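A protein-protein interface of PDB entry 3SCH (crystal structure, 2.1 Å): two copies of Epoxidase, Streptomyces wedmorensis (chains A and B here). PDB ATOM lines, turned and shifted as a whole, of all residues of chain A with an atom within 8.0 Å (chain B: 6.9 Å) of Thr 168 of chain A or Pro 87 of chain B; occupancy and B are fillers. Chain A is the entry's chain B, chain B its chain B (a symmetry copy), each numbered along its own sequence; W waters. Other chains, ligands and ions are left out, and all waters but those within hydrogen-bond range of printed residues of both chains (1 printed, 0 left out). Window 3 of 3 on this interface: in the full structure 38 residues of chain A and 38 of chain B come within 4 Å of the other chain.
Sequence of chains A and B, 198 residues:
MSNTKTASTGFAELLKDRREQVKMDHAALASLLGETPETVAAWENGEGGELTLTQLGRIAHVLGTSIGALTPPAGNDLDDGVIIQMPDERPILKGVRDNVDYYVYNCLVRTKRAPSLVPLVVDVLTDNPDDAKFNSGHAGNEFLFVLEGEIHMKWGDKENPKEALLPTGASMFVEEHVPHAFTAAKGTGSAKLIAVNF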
ATOM      1  N   PHE A 145       7.472   0.369 -18.687  1.00  0.00           N
ATOM      2  CA  PHE A 145       6.418   1.095 -17.985  1.00  0.00           C
ATOM      3  C   PHE A 145       7.093   2.314 -17.325  1.00  0.00           C
ATOM      4  O   PHE A 145       8.131   2.162 -16.678  1.00  0.00           O
ATOM      5  CB  PHE A 145       5.818   0.195 -16.902  1.00  0.00           C
ATOM      6  CG  PHE A 145       4.711   0.843 -16.100  1.00  0.00           C
ATOM      7  CD1 PHE A 145       3.403   0.849 -16.571  1.00  0.00           C
ATOM      8  CD2 PHE A 145       4.977   1.410 -14.858  1.00  0.00           C
ATOM      9  CE1 PHE A 145       2.363   1.407 -15.810  1.00  0.00           C
ATOM     10  CE2 PHE A 145       3.942   1.976 -14.081  1.00  0.00           C
ATOM     11  CZ  PHE A 145       2.634   1.970 -14.559  1.00  0.00           C
ATOM     12  N   VAL A 146       6.510   3.502 -17.493  1.00  0.00           N
ATOM     13  CA  VAL A 146       7.059   4.730 -16.903  1.00  0.00           C
ATOM     14  C   VAL A 146       6.571   4.831 -15.466  1.00  0.00           C
ATOM     15  O   VAL A 146       5.401   5.115 -15.217  1.00  0.00           O
ATOM     16  CB  VAL A 146       6.601   5.991 -17.680  1.00  0.00           C
ATOM     17  CG1 VAL A 146       7.267   7.240 -17.085  1.00  0.00           C
ATOM     18  CG2 VAL A 146       6.973   5.847 -19.168  1.00  0.00           C
ATOM     19  N   LEU A 147       7.475   4.567 -14.531  1.00  0.00           N
ATOM     20  CA  LEU A 147       7.172   4.590 -13.096  1.00  0.00           C
ATOM     21  C   LEU A 147       7.035   5.980 -12.527  1.00  0.00           C
ATOM     22  O   LEU A 147       6.100   6.262 -11.778  1.00  0.00           O
ATOM     23  CB  LEU A 147       8.283   3.911 -12.313  1.00  0.00           C
ATOM     24  CG  LEU A 147       8.134   2.464 -11.907  1.00  0.00           C
ATOM     25  CD1 LEU A 147       9.330   2.124 -11.016  1.00  0.00           C
ATOM     26  CD2 LEU A 147       6.822   2.258 -11.154  1.00  0.00           C
ATOM     27  N   GLU A 148       8.007   6.829 -12.851  1.00  0.00           N
ATOM     28  CA  GLU A 148       8.024   8.203 -12.368  1.00  0.00           C
ATOM     29  C   GLU A 148       8.486   9.167 -13.446  1.00  0.00           C
ATOM     30  O   GLU A 148       9.257   8.793 -14.324  1.00  0.00           O
ATOM     31  CB  GLU A 148       8.971   8.336 -11.184  1.00  0.00           C
ATOM     32  CG  GLU A 148       8.442   7.819  -9.865  1.00  0.00           C
ATOM     33  CD  GLU A 148       9.504   7.862  -8.781  1.00  0.00           C
ATOM     34  OE1 GLU A 148      10.414   8.724  -8.877  1.00  0.00           O
ATOM     35  OE2 GLU A 148       9.427   7.041  -7.837  1.00  0.00           O
ATOM     36  N   GLY A 149       8.009  10.407 -13.358  1.00  0.00           N
ATOM     37  CA  GLY A 149       8.396  11.444 -14.301  1.00  0.00           C
ATOM     38  C   GLY A 149       7.821  11.287 -15.689  1.00  0.00           C
ATOM     39  O   GLY A 149       6.775  10.663 -15.880  1.00  0.00           O
ATOM     40  N   GLU A 150       8.501  11.885 -16.658  1.00  0.00           N
ATOM     41  CA  GLU A 150       8.088  11.807 -18.050  1.00  0.00           C
ATOM     42  C   GLU A 150       9.295  11.414 -18.875  1.00  0.00           C
ATOM     43  O   GLU A 150      10.383  11.975 -18.718  1.00  0.00           O
ATOM     44  CB  GLU A 150       7.534  13.150 -18.525  1.00  0.00           C
ATOM     45  CG  GLU A 150       7.311  13.235 -20.027  1.00  0.00           C
ATOM     46  CD  GLU A 150       6.477  14.442 -20.409  1.00  0.00           C
ATOM     47  OE1 GLU A 150       6.693  15.524 -19.818  1.00  0.00           O
ATOM     48  OE2 GLU A 150       5.611  14.309 -21.298  1.00  0.00           O
ATOM     49  N   ILE A 151       9.096  10.442 -19.755  1.00  0.00           N
ATOM     50  CA  ILE A 151      10.172   9.918 -20.595  1.00  0.00           C
ATOM     51  C   ILE A 151      10.089  10.388 -22.039  1.00  0.00           C
ATOM     52  O   ILE A 151       9.011  10.489 -22.603  1.00  0.00           O
ATOM     53  CB  ILE A 151      10.138   8.362 -20.601  1.00  0.00           C
ATOM     54  CG1 ILE A 151      10.598   7.814 -19.236  1.00  0.00           C
ATOM     55  CG2 ILE A 151      11.006   7.806 -21.734  1.00  0.00           C
ATOM     56  CD1 ILE A 151      12.093   7.975 -18.971  1.00  0.00           C
ATOM     57  N   LEU A 165       6.780  11.152 -26.342  1.00  0.00           N
ATOM     58  CA  LEU A 165       6.865  11.753 -25.011  1.00  0.00           C
ATOM     59  C   LEU A 165       5.928  10.861 -24.224  1.00  0.00           C
ATOM     60  O   LEU A 165       4.765  10.733 -24.572  1.00  0.00           O
ATOM     61  CB  LEU A 165       6.343  13.196 -25.014  1.00  0.00           C
ATOM     62  CG  LEU A 165       7.410  14.259 -25.288  1.00  0.00           C
ATOM     63  CD1 LEU A 165       8.454  14.257 -24.187  1.00  0.00           C
ATOM     64  CD2 LEU A 165       8.087  13.958 -26.596  1.00  0.00           C
ATOM     65  N   LEU A 166       6.439  10.239 -23.169  1.00  0.00           N
ATOM     66  CA  LEU A 166       5.641   9.304 -22.390  1.00  0.00           C
ATOM     67  C   LEU A 166       5.521   9.673 -20.921  1.00  0.00           C
ATOM     68  O   LEU A 166       6.495   9.615 -20.177  1.00  0.00           O
ATOM     69  CB  LEU A 166       6.254   7.901 -22.525  1.00  0.00           C
ATOM     70  CG  LEU A 166       6.465   7.474 -23.988  1.00  0.00           C
ATOM     71  CD1 LEU A 166       7.504   6.357 -24.125  1.00  0.00           C
ATOM     72  CD2 LEU A 166       5.123   7.045 -24.544  1.00  0.00           C
ATOM     73  N   PRO A 167       4.310  10.042 -20.486  1.00  0.00           N
ATOM     74  CA  PRO A 167       4.023  10.419 -19.101  1.00  0.00           C
ATOM     75  C   PRO A 167       4.006   9.180 -18.209  1.00  0.00           C
ATOM     76  O   PRO A 167       4.021   8.047 -18.702  1.00  0.00           O
ATOM     77  CB  PRO A 167       2.649  11.065 -19.205  1.00  0.00           C
ATOM     78  CG  PRO A 167       2.009  10.246 -20.284  1.00  0.00           C
ATOM     79  CD  PRO A 167       3.110  10.174 -21.322  1.00  0.00           C
ATOM     80  N   THR A 168       3.969   9.399 -16.899  1.00  0.00           N
ATOM     81  CA  THR A 168       3.954   8.299 -15.947  1.00  0.00           C
ATOM     82  C   THR A 168       2.726   7.439 -16.206  1.00  0.00           C
ATOM     83  O   THR A 168       1.645   7.953 -16.490  1.00  0.00           O
ATOM     84  CB  THR A 168       3.937   8.823 -14.491  1.00  0.00           C
ATOM     85  OG1 THR A 168       5.110   9.613 -14.267  1.00  0.00           O
ATOM     86  CG2 THR A 168       3.936   7.657 -13.494  1.00  0.00           C
ATOM     87  N   GLY A 169       2.902   6.121 -16.132  1.00  0.00           N
ATOM     88  CA  GLY A 169       1.796   5.222 -16.379  1.00  0.00           C
ATOM     89  C   GLY A 169       1.798   4.725 -17.810  1.00  0.00           C
ATOM     90  O   GLY A 169       1.106   3.748 -18.133  1.00  0.00           O
ATOM     91  N   ALA A 170       2.570   5.371 -18.681  1.00  0.00           N
ATOM     92  CA  ALA A 170       2.616   4.936 -20.083  1.00  0.00           C
ATOM     93  C   ALA A 170       3.346   3.595 -20.179  1.00  0.00           C
ATOM     94  O   ALA A 170       4.230   3.308 -19.372  1.00  0.00           O
ATOM     95  CB  ALA A 170       3.347   5.959 -20.932  1.00  0.00           C
ATOM     96  N   SER A 171       2.988   2.782 -21.165  1.00  0.00           N
ATOM     97  CA  SER A 171       3.669   1.501 -21.343  1.00  0.00           C
ATOM     98  C   SER A 171       4.131   1.352 -22.791  1.00  0.00           C
ATOM     99  O   SER A 171       3.554   1.937 -23.711  1.00  0.00           O
ATOM    100  CB  SER A 171       2.772   0.322 -20.905  1.00  0.00           C
ATOM    101  OG  SER A 171       1.582   0.200 -21.659  1.00  0.00           O
ATOM    102  N   ALA A 191      13.792  10.670 -14.584  1.00  0.00           N
ATOM    103  CA  ALA A 191      12.605   9.838 -14.643  1.00  0.00           C
ATOM    104  C   ALA A 191      12.973   8.402 -14.317  1.00  0.00           C
ATOM    105  O   ALA A 191      14.149   8.061 -14.169  1.00  0.00           O
ATOM    106  CB  ALA A 191      11.964   9.936 -16.030  1.00  0.00           C
ATOM    107  N   LYS A 192      11.960   7.552 -14.228  1.00  0.00           N
ATOM    108  CA  LYS A 192      12.188   6.166 -13.859  1.00  0.00           C
ATOM    109  C   LYS A 192      11.292   5.229 -14.654  1.00  0.00           C
ATOM    110  O   LYS A 192      10.106   5.484 -14.834  1.00  0.00           O
ATOM    111  CB  LYS A 192      11.910   6.028 -12.367  1.00  0.00           C
ATOM    112  CG  LYS A 192      12.511   4.835 -11.717  1.00  0.00           C
ATOM    113  CD  LYS A 192      12.526   5.038 -10.212  1.00  0.00           C
ATOM    114  CE  LYS A 192      13.346   6.263  -9.860  1.00  0.00           C
ATOM    115  NZ  LYS A 192      13.576   6.377  -8.401  1.00  0.00           N
ATOM    116  N   GLN B  85       1.483   2.825 -25.401  1.00  0.00           N
ATOM    117  CA  GLN B  85       0.127   3.020 -24.917  1.00  0.00           C
ATOM    118  C   GLN B  85       0.163   4.083 -23.833  1.00  0.00           C
ATOM    119  O   GLN B  85       0.893   3.947 -22.856  1.00  0.00           O
ATOM    120  CB  GLN B  85      -0.432   1.734 -24.314  1.00  0.00           C
ATOM    121  CG  GLN B  85      -1.885   1.862 -23.878  1.00  0.00           C
ATOM    122  CD  GLN B  85      -2.279   0.821 -22.849  1.00  0.00           C
ATOM    123  OE1 GLN B  85      -1.777   0.826 -21.724  1.00  0.00           O
ATOM    124  NE2 GLN B  85      -3.169  -0.077 -23.227  1.00  0.00           N
ATOM    125  N   MET B  86      -0.624   5.137 -24.024  1.00  0.00           N
ATOM    126  CA  MET B  86      -0.719   6.239 -23.078  1.00  0.00           C
ATOM    127  C   MET B  86      -1.649   5.825 -21.951  1.00  0.00           C
ATOM    128  O   MET B  86      -2.539   5.006 -22.150  1.00  0.00           O
ATOM    129  CB  MET B  86      -1.294   7.466 -23.778  1.00  0.00           C
ATOM    130  CG  MET B  86      -0.483   7.925 -24.981  1.00  0.00           C
ATOM    131  SD  MET B  86       1.255   8.587 -24.470  1.00  0.00           S
ATOM    132  CE  MET B  86       0.711  10.297 -23.790  1.00  0.00           C
ATOM    133  N   PRO B  87      -1.455   6.376 -20.745  1.00  0.00           N
ATOM    134  CA  PRO B  87      -2.335   6.000 -19.639  1.00  0.00           C
ATOM    135  C   PRO B  87      -3.719   6.604 -19.841  1.00  0.00           C
ATOM    136  O   PRO B  87      -3.858   7.648 -20.476  1.00  0.00           O
ATOM    137  CB  PRO B  87      -1.617   6.569 -18.424  1.00  0.00           C
ATOM    138  CG  PRO B  87      -0.960   7.777 -18.969  1.00  0.00           C
ATOM    139  CD  PRO B  87      -0.413   7.312 -20.295  1.00  0.00           C
ATOM    140  N   ASP B  88      -4.739   5.939 -19.310  1.00  0.00           N
ATOM    141  CA  ASP B  88      -6.119   6.410 -19.439  1.00  0.00           C
ATOM    142  C   ASP B  88      -6.767   5.939 -20.744  1.00  0.00           C
ATOM    143  O   ASP B  88      -7.886   6.337 -21.072  1.00  0.00           O
ATOM    144  CB  ASP B  88      -6.188   7.944 -19.340  1.00  0.00           C
ATOM    145  CG  ASP B  88      -5.844   8.459 -17.945  1.00  0.00           C
ATOM    146  OD1 ASP B  88      -6.621   8.193 -17.000  1.00  0.00           O
ATOM    147  OD2 ASP B  88      -4.793   9.128 -17.791  1.00  0.00           O
ATOM    148  N   GLU B  89      -6.050   5.110 -21.497  1.00  0.00           N
ATOM    149  CA  GLU B  89      -6.587   4.547 -22.731  1.00  0.00           C
ATOM    150  C   GLU B  89      -6.387   3.044 -22.587  1.00  0.00           C
ATOM    151  O   GLU B  89      -6.507   2.277 -23.547  1.00  0.00           O
ATOM    152  CB  GLU B  89      -5.844   5.075 -23.963  1.00  0.00           C
ATOM    153  CG  GLU B  89      -4.424   4.574 -24.129  1.00  0.00           C
ATOM    154  CD  GLU B  89      -3.743   5.180 -25.346  1.00  0.00           C
ATOM    155  OE1 GLU B  89      -3.886   6.408 -25.533  1.00  0.00           O
ATOM    156  OE2 GLU B  89      -3.065   4.444 -26.105  1.00  0.00           O
ATOM    157  N   ARG B  90      -6.083   2.642 -21.356  1.00  0.00           N
ATOM    158  CA  ARG B  90      -5.843   1.246 -21.015  1.00  0.00           C
ATOM    159  C   ARG B  90      -7.141   0.560 -20.600  1.00  0.00           C
ATOM    160  O   ARG B  90      -7.948   1.136 -19.862  1.00  0.00           O
ATOM    161  CB  ARG B  90      -4.824   1.157 -19.870  1.00  0.00           C
ATOM    162  CG  ARG B  90      -5.322   1.712 -18.546  1.00  0.00           C
ATOM    163  CD  ARG B  90      -4.321   1.514 -17.404  1.00  0.00           C
ATOM    164  NE  ARG B  90      -3.075   2.260 -17.581  1.00  0.00           N
ATOM    165  CZ  ARG B  90      -2.226   2.531 -16.589  1.00  0.00           C
ATOM    166  NH1 ARG B  90      -2.499   2.122 -15.358  1.00  0.00           N
ATOM    167  NH2 ARG B  90      -1.105   3.199 -16.821  1.00  0.00           N
ATOM    168  N   LEU B 108      -2.293  -2.879 -19.832  1.00  0.00           N
ATOM    169  CA  LEU B 108      -1.250  -2.063 -20.423  1.00  0.00           C
ATOM    170  C   LEU B 108      -1.064  -2.532 -21.868  1.00  0.00           C
ATOM    171  O   LEU B 108      -1.802  -3.383 -22.347  1.00  0.00           O
ATOM    172  CB  LEU B 108       0.051  -2.194 -19.614  1.00  0.00           C
ATOM    173  CG  LEU B 108      -0.138  -1.827 -18.144  1.00  0.00           C
ATOM    174  CD1 LEU B 108       1.128  -2.140 -17.350  1.00  0.00           C
ATOM    175  CD2 LEU B 108      -0.506  -0.352 -18.053  1.00  0.00           C
HETATM  176  O   HOH W   1      -0.298   2.563 -20.395  1.00  0.00           O
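Thr 168 of chain A touches one residue of chain B.
Of chain A, only Pro 167 (3.8 Å), Thr 168 (3.6 Å), Gly 169 (3.9 Å) and Ala 170 (3.9 Å) come within 4 Å of Pro 87 of chain B.
Of the printed residues of chain A, Arg 90 of chain B touches Gly 169 (2.6 Å).
Of the printed residues of chain B, Gly 169 of chain A touches Pro 87 (3.9 Å) and Arg 90 (2.6 Å).
Of the printed residues of chain A, Leu 108 of chain B touches Phe 145 and Ser 171.
Printed residues of chain A within 4 Å of Gln 85 of chain B: Ala 170 and Ser 171.
Glu 148 of chain A touches none of the printed residues of chain B.
The nearest residue of chain A that does not touch Pro 87 of chain B is Ser 171 of chain A (5.7 Å).
The nearest printed residue of chain B that does not touch Phe 145 of chain A is Arg 90 of chain B (4.03 Å).
Printed residues of chain B that touch a printed residue of chain A: Gln 85, Met 86, Pro 87, Arg 90 and Leu 108.
Of the 16 printed residues of chain A, 6 touch a printed residue of chain B.
Hydrophobic or aromatic side chains of chain A within 4 Å of the printed part of chain B: Phe 145, Pro 167 and Ala 170.
Among the printed residues, no Asp or Glu carboxylate lies within 4 Å of a Lys or Arg side-chain nitrogen of the other chain.
The backbone carbonyl oxygen of Val 146 of chain A sits at hydrogen-bond distance from the backbone NH of Gly 169 of chain A, at 2.8 Å.
The backbone NH (N) of Val 146 of chain A sits at hydrogen-bond distance from the backbone carbonyl oxygen (O) of Ala 170 of chain A, at 3.0 Å.
OG1 of Thr 168 of chain A lies within hydrogen-bond range of O of Gly 149 of chain A, 2.5 Å away.
The backbone NH (N) of Met 86 of chain B sits at hydrogen-bond distance from the side-chain carboxylate (OE2) of Glu 89 of chain B, at 3.3 Å.
The backbone carbonyl oxygen of Gly 169 of chain A lies within hydrogen-bond range of the guanidinium group of Arg 90 of chain B, 2.6 Å away.
O of Ser 171 of chain A is in hydrogen-bond range of N of Gln 85 of chain B.
Among the printed residues, pairs that only touch across the chains: Ala 170 of chain A with Gln 85 of chain B, Pro 167 of chain A with Met 86 of chain B, Ser 171 of chain A with Leu 108 of chain B, Thr 168 of chain A with Pro 87 of chain B, Pro 167 of chain A with Pro 87 of chain B, Phe 145 of chain A with Leu 108 of chain B, Ala 170 of chain A with Pro 87 of chain B and Gly 169 of chain A with Pro 87 of chain B.
Water W1 lies within hydrogen-bond range of the side-chain amide oxygen (OE1) of Gln 85 of chain B, the backbone carbonyl oxygen (O) of Gly 169 of chain A and the side-chain hydroxyl (OG) of Ser 171 of chain A.
No position is printed for both chains.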
